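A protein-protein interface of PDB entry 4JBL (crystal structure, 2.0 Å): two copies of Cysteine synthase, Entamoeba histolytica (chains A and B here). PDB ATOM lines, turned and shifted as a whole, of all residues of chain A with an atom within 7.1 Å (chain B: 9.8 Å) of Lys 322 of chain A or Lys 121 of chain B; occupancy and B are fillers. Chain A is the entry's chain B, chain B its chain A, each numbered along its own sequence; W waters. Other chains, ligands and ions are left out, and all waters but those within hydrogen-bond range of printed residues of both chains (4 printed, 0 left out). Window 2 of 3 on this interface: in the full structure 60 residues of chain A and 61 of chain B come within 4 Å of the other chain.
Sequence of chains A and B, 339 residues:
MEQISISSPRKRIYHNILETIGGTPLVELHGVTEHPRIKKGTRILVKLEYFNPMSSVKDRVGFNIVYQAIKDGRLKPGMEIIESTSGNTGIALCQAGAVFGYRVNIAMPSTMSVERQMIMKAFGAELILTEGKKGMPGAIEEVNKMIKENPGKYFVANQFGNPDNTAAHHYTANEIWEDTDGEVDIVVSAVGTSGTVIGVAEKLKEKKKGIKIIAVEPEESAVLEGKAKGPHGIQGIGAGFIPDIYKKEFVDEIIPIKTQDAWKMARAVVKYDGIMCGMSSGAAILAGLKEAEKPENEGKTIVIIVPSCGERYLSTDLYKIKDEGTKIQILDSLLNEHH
Water W1 bridges O of Ala 122 of chain B (2.6 Å) and O of Arg 267 of chain A (2.9 Å). Water W2 bridges the backbone carbonyl oxygen (O) of Ala 98 of chain B (2.8 Å) and the backbone carbonyl oxygen (O) of Lys 271 of chain A (2.9 Å). Water W3 lies within hydrogen-bond range of the backbone carbonyl oxygen (O) of Phe 123 of chain B and the backbone carbonyl oxygen (O) of Lys 271 of chain A. Water W4 lies within hydrogen-bond range of the backbone NH (N) of Tyr 319 of chain A (2.8 Å) and the side-chain sulfur (SD) of Met 118 of chain B (3.3 Å).
Of the printed residues of chain B, Val 270 of chain A touches Ala 122 (3.5 Å) and Phe 123 (3.7 Å). Of the printed residues of chain B, Lys 271 of chain A touches Ala 122 (3.9 Å). Of the printed residues of chain B, Tyr 319 of chain A touches Ala 122. No residue of chain B comes within 4 Å of Ile 321 of chain A. Printed residues of chain B within 4 Å of Lys 322 of chain A: Lys 121. Of the printed residues of chain A, Lys 121 of chain B touches Lys 322. Of the printed residues of chain A, Ala 122 of chain B touches Val 270 (3.5 Å), Lys 271 (3.9 Å) and Tyr 319 (3.7 Å). Of the printed residues of chain A, Phe 123 of chain B touches Val 270 (3.7 Å). The nearest printed residue of chain B that does not touch Lys 322 of chain A is Met 118 of chain B (6.7 Å). The nearest printed residue of chain B that does not touch Val 270 of chain A is Ala 98 of chain B (4.4 Å).
No position is printed for both chains. Of the 5 pairs that touch across the chains among the printed residues, none has its exchanged pair printed and touching as well.
Ala 122 of chain B touches Val 270 of chain A. Phe 123 of chain B touches Val 270 of chain A. Lys 271 of chain A touches Ala 122 of chain B. CB of Ala 122 of chain B touches CD1 of Tyr 319 of chain A (3.7 Å). NZ of Lys 322 of chain A touches CE of Lys 121 of chain B (3.998 Å).
Printed residues of chain A that touch a printed residue of chain B: Val 270, Lys 271, Tyr 319 and Lys 322. Among the printed residues, 5 pairs touch across the chains. Among the printed residues, no Asp or Glu carboxylate lies within 4 Å of a Lys or Arg side-chain nitrogen of the other chain.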
ATOM      1  N   ARG A 267      17.457 -15.205 -10.833  1.00  0.00           N
ATOM      2  CA  ARG A 267      16.653 -14.805  -9.713  1.00  0.00           C
ATOM      3  C   ARG A 267      16.045 -16.007  -8.984  1.00  0.00           C
ATOM      4  O   ARG A 267      16.049 -16.073  -7.791  1.00  0.00           O
ATOM      5  CB  ARG A 267      15.588 -13.835 -10.177  1.00  0.00           C
ATOM      6  CG  ARG A 267      16.068 -12.417 -10.153  1.00  0.00           C
ATOM      7  CD  ARG A 267      14.903 -11.458 -10.231  1.00  0.00           C
ATOM      8  NE  ARG A 267      15.160 -10.807 -11.426  1.00  0.00           N
ATOM      9  CZ  ARG A 267      14.551 -10.993 -12.552  1.00  0.00           C
ATOM     10  NH1 ARG A 267      13.524 -11.727 -12.637  1.00  0.00           N
ATOM     11  NH2 ARG A 267      14.998 -10.358 -13.563  1.00  0.00           N
ATOM     12  N   VAL A 270      18.822 -18.272  -6.975  1.00  0.00           N
ATOM     13  CA  VAL A 270      19.214 -17.781  -5.616  1.00  0.00           C
ATOM     14  C   VAL A 270      18.035 -17.893  -4.659  1.00  0.00           C
ATOM     15  O   VAL A 270      18.195 -18.306  -3.491  1.00  0.00           O
ATOM     16  CB  VAL A 270      19.855 -16.404  -5.632  1.00  0.00           C
ATOM     17  CG1 VAL A 270      18.947 -15.370  -6.287  1.00  0.00           C
ATOM     18  CG2 VAL A 270      20.357 -15.995  -4.228  1.00  0.00           C
ATOM     19  N   LYS A 271      16.825 -17.656  -5.142  1.00  0.00           N
ATOM     20  CA  LYS A 271      15.663 -17.753  -4.200  1.00  0.00           C
ATOM     21  C   LYS A 271      15.339 -19.223  -3.779  1.00  0.00           C
ATOM     22  O   LYS A 271      15.165 -19.486  -2.585  1.00  0.00           O
ATOM     23  CB  LYS A 271      14.460 -17.031  -4.762  1.00  0.00           C
ATOM     24  CG  LYS A 271      13.210 -16.925  -3.841  1.00  0.00           C
ATOM     25  CD  LYS A 271      12.147 -16.077  -4.575  1.00  0.00           C
ATOM     26  CE  LYS A 271      10.766 -16.176  -3.918  1.00  0.00           C
ATOM     27  NZ  LYS A 271      10.708 -15.161  -2.844  1.00  0.00           N
ATOM     28  N   TYR A 319      18.854  -7.947 -10.374  1.00  0.00           N
ATOM     29  CA  TYR A 319      17.900  -8.108  -9.251  1.00  0.00           C
ATOM     30  C   TYR A 319      16.866  -6.942  -9.213  1.00  0.00           C
ATOM     31  O   TYR A 319      16.198  -6.756  -8.202  1.00  0.00           O
ATOM     32  CB  TYR A 319      18.634  -8.273  -7.886  1.00  0.00           C
ATOM     33  CG  TYR A 319      19.637  -9.450  -7.891  1.00  0.00           C
ATOM     34  CD1 TYR A 319      19.177 -10.761  -7.968  1.00  0.00           C
ATOM     35  CD2 TYR A 319      21.025  -9.230  -7.904  1.00  0.00           C
ATOM     36  CE1 TYR A 319      20.052 -11.835  -8.021  1.00  0.00           C
ATOM     37  CE2 TYR A 319      21.916 -10.305  -7.924  1.00  0.00           C
ATOM     38  CZ  TYR A 319      21.422 -11.597  -7.980  1.00  0.00           C
ATOM     39  OH  TYR A 319      22.230 -12.720  -8.000  1.00  0.00           O
ATOM     40  N   LYS A 320      16.733  -6.206 -10.319  1.00  0.00           N
ATOM     41  CA  LYS A 320      15.740  -5.122 -10.415  1.00  0.00           C
ATOM     42  C   LYS A 320      14.288  -5.637 -10.445  1.00  0.00           C
ATOM     43  O   LYS A 320      13.543  -5.444  -9.482  1.00  0.00           O
ATOM     44  CB  LYS A 320      16.022  -4.225 -11.621  1.00  0.00           C
ATOM     45  CG  LYS A 320      15.350  -2.865 -11.510  1.00  0.00           C
ATOM     46  CD  LYS A 320      15.690  -1.987 -12.705  1.00  0.00           C
ATOM     47  CE  LYS A 320      14.763  -0.788 -12.852  1.00  0.00           C
ATOM     48  NZ  LYS A 320      15.107  -0.148 -14.153  1.00  0.00           N
ATOM     49  N   ILE A 321      13.886  -6.313 -11.515  1.00  0.00           N
ATOM     50  CA  ILE A 321      12.462  -6.669 -11.646  1.00  0.00           C
ATOM     51  C   ILE A 321      12.079  -7.749 -10.683  1.00  0.00           C
ATOM     52  O   ILE A 321      12.903  -8.597 -10.335  1.00  0.00           O
ATOM     53  CB  ILE A 321      11.937  -6.864 -13.115  1.00  0.00           C
ATOM     54  CG1 ILE A 321      12.405  -8.153 -13.769  1.00  0.00           C
ATOM     55  CG2 ILE A 321      12.297  -5.672 -14.009  1.00  0.00           C
ATOM     56  CD1 ILE A 321      12.448  -8.024 -15.287  1.00  0.00           C
ATOM     57  N   LYS A 322      10.854  -7.663 -10.175  1.00  0.00           N
ATOM     58  CA  LYS A 322      10.373  -8.651  -9.221  1.00  0.00           C
ATOM     59  C   LYS A 322       9.377  -9.539  -9.950  1.00  0.00           C
ATOM     60  O   LYS A 322       8.407  -9.063 -10.544  1.00  0.00           O
ATOM     61  CB  LYS A 322       9.757  -7.996  -7.963  1.00  0.00           C
ATOM     62  CG  LYS A 322      10.457  -6.733  -7.456  1.00  0.00           C
ATOM     63  CD  LYS A 322      11.859  -6.974  -6.896  1.00  0.00           C
ATOM     64  CE  LYS A 322      12.473  -5.666  -6.391  1.00  0.00           C
ATOM     65  NZ  LYS A 322      13.772  -5.813  -5.666  1.00  0.00           N
ATOM     66  N   ASP A 323       9.638 -10.835  -9.934  1.00  0.00           N
ATOM     67  CA  ASP A 323       8.781 -11.772 -10.614  1.00  0.00           C
ATOM     68  C   ASP A 323       7.501 -12.028  -9.792  1.00  0.00           C
ATOM     69  O   ASP A 323       7.540 -12.098  -8.560  1.00  0.00           O
ATOM     70  CB  ASP A 323       9.536 -13.075 -10.792  1.00  0.00           C
ATOM     71  CG  ASP A 323      10.853 -12.876 -11.455  1.00  0.00           C
ATOM     72  OD1 ASP A 323      10.899 -12.370 -12.580  1.00  0.00           O
ATOM     73  OD2 ASP A 323      11.873 -13.184 -10.836  1.00  0.00           O
ATOM     74  N   GLU A 324       6.389 -12.181 -10.496  1.00  0.00           N
ATOM     75  CA  GLU A 324       5.113 -12.489  -9.887  1.00  0.00           C
ATOM     76  C   GLU A 324       4.962 -13.979  -9.898  1.00  0.00           C
ATOM     77  O   GLU A 324       5.571 -14.657 -10.725  1.00  0.00           O
ATOM     78  CB  GLU A 324       3.979 -11.857 -10.708  1.00  0.00           C
ATOM     79  CG  GLU A 324       2.976 -11.091  -9.873  1.00  0.00           C
ATOM     80  CD  GLU A 324       3.587  -9.816  -9.308  1.00  0.00           C
ATOM     81  OE1 GLU A 324       3.539  -8.793 -10.019  1.00  0.00           O
ATOM     82  OE2 GLU A 324       4.122  -9.831  -8.164  1.00  0.00           O
ATOM     83  N   GLY A 325       4.164 -14.494  -8.973  1.00  0.00           N
ATOM     84  CA  GLY A 325       3.745 -15.880  -9.006  1.00  0.00           C
ATOM     85  C   GLY A 325       4.406 -16.712  -7.937  1.00  0.00           C
ATOM     86  O   GLY A 325       5.362 -16.262  -7.298  1.00  0.00           O
ATOM     87  N   ILE A 330       6.653 -19.440 -11.771  1.00  0.00           N
ATOM     88  CA  ILE A 330       7.870 -18.836 -12.305  1.00  0.00           C
ATOM     89  C   ILE A 330       8.599 -19.850 -13.208  1.00  0.00           C
ATOM     90  O   ILE A 330       9.056 -19.507 -14.325  1.00  0.00           O
ATOM     91  CB  ILE A 330       8.734 -18.276 -11.159  1.00  0.00           C
ATOM     92  CG1 ILE A 330       8.143 -16.911 -10.714  1.00  0.00           C
ATOM     93  CG2 ILE A 330      10.201 -18.137 -11.592  1.00  0.00           C
ATOM     94  CD1 ILE A 330       8.517 -16.495  -9.299  1.00  0.00           C
ATOM     95  N   GLY B  90      23.838 -11.457   8.295  1.00  0.00           N
ATOM     96  CA  GLY B  90      22.549 -11.372   7.578  1.00  0.00           C
ATOM     97  C   GLY B  90      22.558 -12.252   6.327  1.00  0.00           C
ATOM     98  O   GLY B  90      21.627 -13.093   6.116  1.00  0.00           O
ATOM     99  N   ILE B  91      23.618 -12.117   5.514  1.00  0.00           N
ATOM    100  CA  ILE B  91      23.704 -12.885   4.251  1.00  0.00           C
ATOM    101  C   ILE B  91      23.708 -14.389   4.564  1.00  0.00           C
ATOM    102  O   ILE B  91      23.120 -15.222   3.862  1.00  0.00           O
ATOM    103  CB  ILE B  91      25.001 -12.420   3.517  1.00  0.00           C
ATOM    104  CG1 ILE B  91      24.817 -10.959   3.009  1.00  0.00           C
ATOM    105  CG2 ILE B  91      25.313 -13.351   2.351  1.00  0.00           C
ATOM    106  CD1 ILE B  91      26.163 -10.247   2.737  1.00  0.00           C
ATOM    107  N   CYS B  94      20.311 -15.692   5.471  1.00  0.00           N
ATOM    108  CA  CYS B  94      19.490 -15.794   4.269  1.00  0.00           C
ATOM    109  C   CYS B  94      19.816 -17.044   3.439  1.00  0.00           C
ATOM    110  O   CYS B  94      18.951 -17.775   2.968  1.00  0.00           O
ATOM    111  CB  CYS B  94      19.724 -14.538   3.410  1.00  0.00           C
ATOM    112  SG  CYS B  94      19.049 -12.992   4.029  1.00  0.00           S
ATOM    113  N   GLN B  95      21.091 -17.280   3.254  1.00  0.00           N
ATOM    114  CA  GLN B  95      21.532 -18.518   2.628  1.00  0.00           C
ATOM    115  C   GLN B  95      20.929 -19.768   3.310  1.00  0.00           C
ATOM    116  O   GLN B  95      20.284 -20.615   2.671  1.00  0.00           O
ATOM    117  CB  GLN B  95      23.077 -18.567   2.656  1.00  0.00           C
ATOM    118  CG  GLN B  95      23.683 -19.794   1.978  1.00  0.00           C
ATOM    119  CD  GLN B  95      25.209 -19.694   1.825  1.00  0.00           C
ATOM    120  OE1 GLN B  95      25.675 -19.627   0.714  1.00  0.00           O
ATOM    121  NE2 GLN B  95      25.977 -19.647   2.938  1.00  0.00           N
ATOM    122  N   ALA B  98      17.107 -19.958   2.991  1.00  0.00           N
ATOM    123  CA  ALA B  98      16.789 -20.351   1.598  1.00  0.00           C
ATOM    124  C   ALA B  98      16.828 -21.864   1.435  1.00  0.00           C
ATOM    125  O   ALA B  98      15.885 -22.441   0.871  1.00  0.00           O
ATOM    126  CB  ALA B  98      17.756 -19.699   0.625  1.00  0.00           C
ATOM    127  N   VAL B 104      13.255 -15.413   6.342  1.00  0.00           N
ATOM    128  CA  VAL B 104      14.297 -14.688   7.009  1.00  0.00           C
ATOM    129  C   VAL B 104      13.950 -13.215   7.008  1.00  0.00           C
ATOM    130  O   VAL B 104      13.646 -12.574   5.947  1.00  0.00           O
ATOM    131  CB  VAL B 104      15.708 -14.906   6.375  1.00  0.00           C
ATOM    132  CG1 VAL B 104      16.767 -14.204   7.176  1.00  0.00           C
ATOM    133  CG2 VAL B 104      16.007 -16.413   6.320  1.00  0.00           C
ATOM    134  N   ASN B 105      13.981 -12.659   8.207  1.00  0.00           N
ATOM    135  CA  ASN B 105      13.693 -11.238   8.357  1.00  0.00           C
ATOM    136  C   ASN B 105      14.930 -10.579   8.848  1.00  0.00           C
ATOM    137  O   ASN B 105      15.434 -10.931   9.902  1.00  0.00           O
ATOM    138  CB  ASN B 105      12.574 -11.008   9.423  1.00  0.00           C
ATOM    139  CG  ASN B 105      11.301 -11.689   9.044  1.00  0.00           C
ATOM    140  OD1 ASN B 105      10.460 -11.086   8.345  1.00  0.00           O
ATOM    141  ND2 ASN B 105      11.149 -12.967   9.434  1.00  0.00           N
ATOM    142  N   ILE B 106      15.435  -9.598   8.111  1.00  0.00           N
ATOM    143  CA  ILE B 106      16.643  -8.961   8.573  1.00  0.00           C
ATOM    144  C   ILE B 106      16.443  -7.450   8.817  1.00  0.00           C
ATOM    145  O   ILE B 106      15.968  -6.734   7.935  1.00  0.00           O
ATOM    146  CB  ILE B 106      17.792  -9.141   7.565  1.00  0.00           C
ATOM    147  CG1 ILE B 106      18.193 -10.656   7.369  1.00  0.00           C
ATOM    148  CG2 ILE B 106      18.952  -8.258   7.995  1.00  0.00           C
ATOM    149  CD1 ILE B 106      18.871 -11.365   8.538  1.00  0.00           C
ATOM    150  N   MET B 108      17.893  -3.660   9.654  1.00  0.00           N
ATOM    151  CA  MET B 108      19.084  -2.809   9.680  1.00  0.00           C
ATOM    152  C   MET B 108      18.719  -1.342   9.398  1.00  0.00           C
ATOM    153  O   MET B 108      17.654  -1.076   8.813  1.00  0.00           O
ATOM    154  CB  MET B 108      20.044  -3.248   8.581  1.00  0.00           C
ATOM    155  CG  MET B 108      19.449  -3.061   7.151  1.00  0.00           C
ATOM    156  SD  MET B 108      20.589  -3.850   5.936  1.00  0.00           S
ATOM    157  CE  MET B 108      19.745  -5.396   5.710  1.00  0.00           C
ATOM    158  N   SER B 113      24.720  -0.227   4.071  1.00  0.00           N
ATOM    159  CA  SER B 113      25.021  -1.367   3.172  1.00  0.00           C
ATOM    160  C   SER B 113      23.877  -1.769   2.239  1.00  0.00           C
ATOM    161  O   SER B 113      23.399  -2.937   2.255  1.00  0.00           O
ATOM    162  CB  SER B 113      25.520  -2.608   3.961  1.00  0.00           C
ATOM    163  OG  SER B 113      26.918  -2.544   4.238  1.00  0.00           O
ATOM    164  N   VAL B 114      23.475  -0.815   1.403  1.00  0.00           N
ATOM    165  CA  VAL B 114      22.440  -1.040   0.374  1.00  0.00           C
ATOM    166  C   VAL B 114      22.850  -2.113  -0.708  1.00  0.00           C
ATOM    167  O   VAL B 114      21.994  -2.721  -1.414  1.00  0.00           O
ATOM    168  CB  VAL B 114      22.185   0.302  -0.269  1.00  0.00           C
ATOM    169  CG1 VAL B 114      23.530   1.001  -0.396  1.00  0.00           C
ATOM    170  CG2 VAL B 114      21.460   0.155  -1.593  1.00  0.00           C
ATOM    171  N   GLU B 115      24.156  -2.330  -0.869  1.00  0.00           N
ATOM    172  CA  GLU B 115      24.586  -3.490  -1.669  1.00  0.00           C
ATOM    173  C   GLU B 115      24.156  -4.722  -0.892  1.00  0.00           C
ATOM    174  O   GLU B 115      23.508  -5.616  -1.440  1.00  0.00           O
ATOM    175  CB  GLU B 115      26.096  -3.485  -1.999  1.00  0.00           C
ATOM    176  CG  GLU B 115      26.936  -2.320  -1.440  1.00  0.00           C
ATOM    177  CD  GLU B 115      27.703  -2.686  -0.168  1.00  0.00           C
ATOM    178  OE1 GLU B 115      28.435  -3.718  -0.153  1.00  0.00           O
ATOM    179  OE2 GLU B 115      27.576  -1.939   0.826  1.00  0.00           O
ATOM    180  N   ARG B 116      24.452  -4.745   0.409  1.00  0.00           N
ATOM    181  CA  ARG B 116      24.124  -5.950   1.199  1.00  0.00           C
ATOM    182  C   ARG B 116      22.601  -6.133   1.325  1.00  0.00           C
ATOM    183  O   ARG B 116      22.115  -7.259   1.375  1.00  0.00           O
ATOM    184  CB  ARG B 116      24.861  -6.000   2.553  1.00  0.00           C
ATOM    185  CG  ARG B 116      26.363  -6.290   2.456  1.00  0.00           C
ATOM    186  CD  ARG B 116      26.994  -6.666   3.814  1.00  0.00           C
ATOM    187  NE  ARG B 116      27.804  -5.573   4.388  1.00  0.00           N
ATOM    188  CZ  ARG B 116      29.099  -5.666   4.717  1.00  0.00           C
ATOM    189  NH1 ARG B 116      29.772  -6.804   4.560  1.00  0.00           N
ATOM    190  NH2 ARG B 116      29.733  -4.615   5.223  1.00  0.00           N
ATOM    191  N   GLN B 117      21.855  -5.032   1.310  1.00  0.00           N
ATOM    192  CA  GLN B 117      20.402  -5.114   1.162  1.00  0.00           C
ATOM    193  C   GLN B 117      19.923  -5.909  -0.029  1.00  0.00           C
ATOM    194  O   GLN B 117      18.973  -6.694   0.067  1.00  0.00           O
ATOM    195  CB  GLN B 117      19.787  -3.725   1.067  1.00  0.00           C
ATOM    196  CG  GLN B 117      19.918  -3.021   2.410  1.00  0.00           C
ATOM    197  CD  GLN B 117      19.313  -1.669   2.434  1.00  0.00           C
ATOM    198  OE1 GLN B 117      18.335  -1.398   1.757  1.00  0.00           O
ATOM    199  NE2 GLN B 117      19.867  -0.813   3.301  1.00  0.00           N
ATOM    200  N   MET B 118      20.533  -5.601  -1.175  1.00  0.00           N
ATOM    201  CA  MET B 118      20.162  -6.196  -2.432  1.00  0.00           C
ATOM    202  C   MET B 118      20.466  -7.680  -2.371  1.00  0.00           C
ATOM    203  O   MET B 118      19.638  -8.454  -2.794  1.00  0.00           O
ATOM    204  CB  MET B 118      21.007  -5.593  -3.591  1.00  0.00           C
ATOM    205  CG  MET B 118      20.722  -6.311  -4.929  1.00  0.00           C
ATOM    206  SD  MET B 118      21.239  -5.387  -6.399  1.00  0.00           S
ATOM    207  CE  MET B 118      20.153  -3.911  -6.254  1.00  0.00           C
ATOM    208  N   ILE B 119      21.659  -8.059  -1.862  1.00  0.00           N
ATOM    209  CA  ILE B 119      22.052  -9.470  -1.735  1.00  0.00           C
ATOM    210  C   ILE B 119      20.958 -10.184  -0.905  1.00  0.00           C
ATOM    211  O   ILE B 119      20.371 -11.193  -1.310  1.00  0.00           O
ATOM    212  CB  ILE B 119      23.445  -9.643  -1.057  1.00  0.00           C
ATOM    213  CG1 ILE B 119      24.608  -9.028  -1.898  1.00  0.00           C
ATOM    214  CG2 ILE B 119      23.750 -11.119  -0.923  1.00  0.00           C
ATOM    215  CD1 ILE B 119      25.909  -8.861  -1.132  1.00  0.00           C
ATOM    216  N   MET B 120      20.645  -9.605   0.230  1.00  0.00           N
ATOM    217  CA  MET B 120      19.650 -10.244   1.141  1.00  0.00           C
ATOM    218  C   MET B 120      18.269 -10.441   0.525  1.00  0.00           C
ATOM    219  O   MET B 120      17.667 -11.541   0.562  1.00  0.00           O
ATOM    220  CB  MET B 120      19.670  -9.552   2.504  1.00  0.00           C
ATOM    221  CG  MET B 120      20.916  -9.963   3.295  1.00  0.00           C
ATOM    222  SD  MET B 120      20.967  -9.179   4.883  1.00  0.00           S
ATOM    223  CE  MET B 120      21.760  -7.611   4.556  1.00  0.00           C
ATOM    224  N   LYS B 121      17.793  -9.394  -0.104  1.00  0.00           N
ATOM    225  CA  LYS B 121      16.541  -9.442  -0.836  1.00  0.00           C
ATOM    226  C   LYS B 121      16.573 -10.485  -1.952  1.00  0.00           C
ATOM    227  O   LYS B 121      15.590 -11.148  -2.164  1.00  0.00           O
ATOM    228  CB  LYS B 121      16.261  -8.092  -1.489  1.00  0.00           C
ATOM    229  CG  LYS B 121      15.298  -7.227  -0.689  1.00  0.00           C
ATOM    230  CD  LYS B 121      15.679  -5.756  -0.799  1.00  0.00           C
ATOM    231  CE  LYS B 121      14.974  -5.044  -1.931  1.00  0.00           C
ATOM    232  NZ  LYS B 121      13.566  -4.806  -1.506  1.00  0.00           N
ATOM    233  N   ALA B 122      17.698 -10.612  -2.661  1.00  0.00           N
ATOM    234  CA  ALA B 122      17.820 -11.623  -3.721  1.00  0.00           C
ATOM    235  C   ALA B 122      17.605 -13.051  -3.164  1.00  0.00           C
ATOM    236  O   ALA B 122      16.981 -13.942  -3.810  1.00  0.00           O
ATOM    237  CB  ALA B 122      19.181 -11.454  -4.366  1.00  0.00           C
ATOM    238  N   PHE B 123      18.044 -13.254  -1.915  1.00  0.00           N
ATOM    239  CA  PHE B 123      17.872 -14.516  -1.272  1.00  0.00           C
ATOM    240  C   PHE B 123      16.451 -14.697  -0.718  1.00  0.00           C
ATOM    241  O   PHE B 123      16.157 -15.715  -0.066  1.00  0.00           O
ATOM    242  CB  PHE B 123      18.894 -14.625  -0.122  1.00  0.00           C
ATOM    243  CG  PHE B 123      20.196 -15.194  -0.532  1.00  0.00           C
ATOM    244  CD1 PHE B 123      20.391 -16.558  -0.472  1.00  0.00           C
ATOM    245  CD2 PHE B 123      21.228 -14.391  -0.963  1.00  0.00           C
ATOM    246  CE1 PHE B 123      21.631 -17.121  -0.851  1.00  0.00           C
ATOM    247  CE2 PHE B 123      22.454 -14.944  -1.344  1.00  0.00           C
ATOM    248  CZ  PHE B 123      22.639 -16.307  -1.330  1.00  0.00           C
ATOM    249  N   GLY B 124      15.565 -13.733  -0.966  1.00  0.00           N
ATOM    250  CA  GLY B 124      14.195 -13.855  -0.460  1.00  0.00           C
ATOM    251  C   GLY B 124      13.897 -13.266   0.931  1.00  0.00           C
ATOM    252  O   GLY B 124      12.825 -13.496   1.461  1.00  0.00           O
ATOM    253  N   ALA B 125      14.819 -12.534   1.517  1.00  0.00           N
ATOM    254  CA  ALA B 125      14.651 -12.005   2.880  1.00  0.00           C
ATOM    255  C   ALA B 125      13.627 -10.871   2.878  1.00  0.00           C
ATOM    256  O   ALA B 125      13.492 -10.185   1.865  1.00  0.00           O
ATOM    257  CB  ALA B 125      15.970 -11.469   3.380  1.00  0.00           C
ATOM    258  N   GLU B 126      12.891 -10.713   3.986  1.00  0.00           N
ATOM    259  CA  GLU B 126      12.174  -9.463   4.243  1.00  0.00           C
ATOM    260  C   GLU B 126      13.146  -8.546   4.914  1.00  0.00           C
ATOM    261  O   GLU B 126      13.655  -8.894   5.942  1.00  0.00           O
ATOM    262  CB  GLU B 126      10.998  -9.665   5.242  1.00  0.00           C
ATOM    263  CG  GLU B 126       9.721 -10.302   4.701  1.00  0.00           C
ATOM    264  CD  GLU B 126       8.763 -10.760   5.832  1.00  0.00           C
ATOM    265  OE1 GLU B 126       8.731 -11.983   6.193  1.00  0.00           O
ATOM    266  OE2 GLU B 126       8.050  -9.886   6.390  1.00  0.00           O
ATOM    267  N   LEU B 127      13.378  -7.346   4.393  1.00  0.00           N
ATOM    268  CA  LEU B 127      14.194  -6.405   5.110  1.00  0.00           C
ATOM    269  C   LEU B 127      13.333  -5.498   5.985  1.00  0.00           C
ATOM    270  O   LEU B 127      12.326  -4.982   5.551  1.00  0.00           O
ATOM    271  CB  LEU B 127      15.016  -5.560   4.164  1.00  0.00           C
ATOM    272  CG  LEU B 127      16.037  -6.356   3.361  1.00  0.00           C
ATOM    273  CD1 LEU B 127      16.931  -5.401   2.593  1.00  0.00           C
ATOM    274  CD2 LEU B 127      16.892  -7.228   4.267  1.00  0.00           C
ATOM    275  N   ILE B 128      13.754  -5.314   7.222  1.00  0.00           N
ATOM    276  CA  ILE B 128      13.106  -4.400   8.167  1.00  0.00           C
ATOM    277  C   ILE B 128      14.017  -3.180   8.236  1.00  0.00           C
ATOM    278  O   ILE B 128      15.068  -3.168   8.913  1.00  0.00           O
ATOM    279  CB  ILE B 128      12.949  -5.146   9.521  1.00  0.00           C
ATOM    280  CG1 ILE B 128      11.924  -6.259   9.331  1.00  0.00           C
ATOM    281  CG2 ILE B 128      12.545  -4.183  10.635  1.00  0.00           C
ATOM    282  CD1 ILE B 128      11.970  -7.331  10.361  1.00  0.00           C
ATOM    283  N   LEU B 129      13.704  -2.148   7.477  1.00  0.00           N
ATOM    284  CA  LEU B 129      14.634  -1.008   7.421  1.00  0.00           C
ATOM    285  C   LEU B 129      14.296   0.058   8.451  1.00  0.00           C
ATOM    286  O   LEU B 129      13.230   0.649   8.388  1.00  0.00           O
ATOM    287  CB  LEU B 129      14.729  -0.454   5.989  1.00  0.00           C
ATOM    288  CG  LEU B 129      15.244  -1.447   4.916  1.00  0.00           C
ATOM    289  CD1 LEU B 129      15.288  -0.824   3.497  1.00  0.00           C
ATOM    290  CD2 LEU B 129      16.603  -1.999   5.306  1.00  0.00           C
HETATM  291  O   HOH W   1      16.021 -13.655  -6.215  1.00  0.00           O
HETATM  292  O   HOH W   2      13.915 -21.309  -0.777  1.00  0.00           O
HETATM  293  O   HOH W   3      14.459 -17.948  -0.270  1.00  0.00           O
HETATM  294  O   HOH W   4      20.776  -6.007  -9.646  1.00  0.00           O
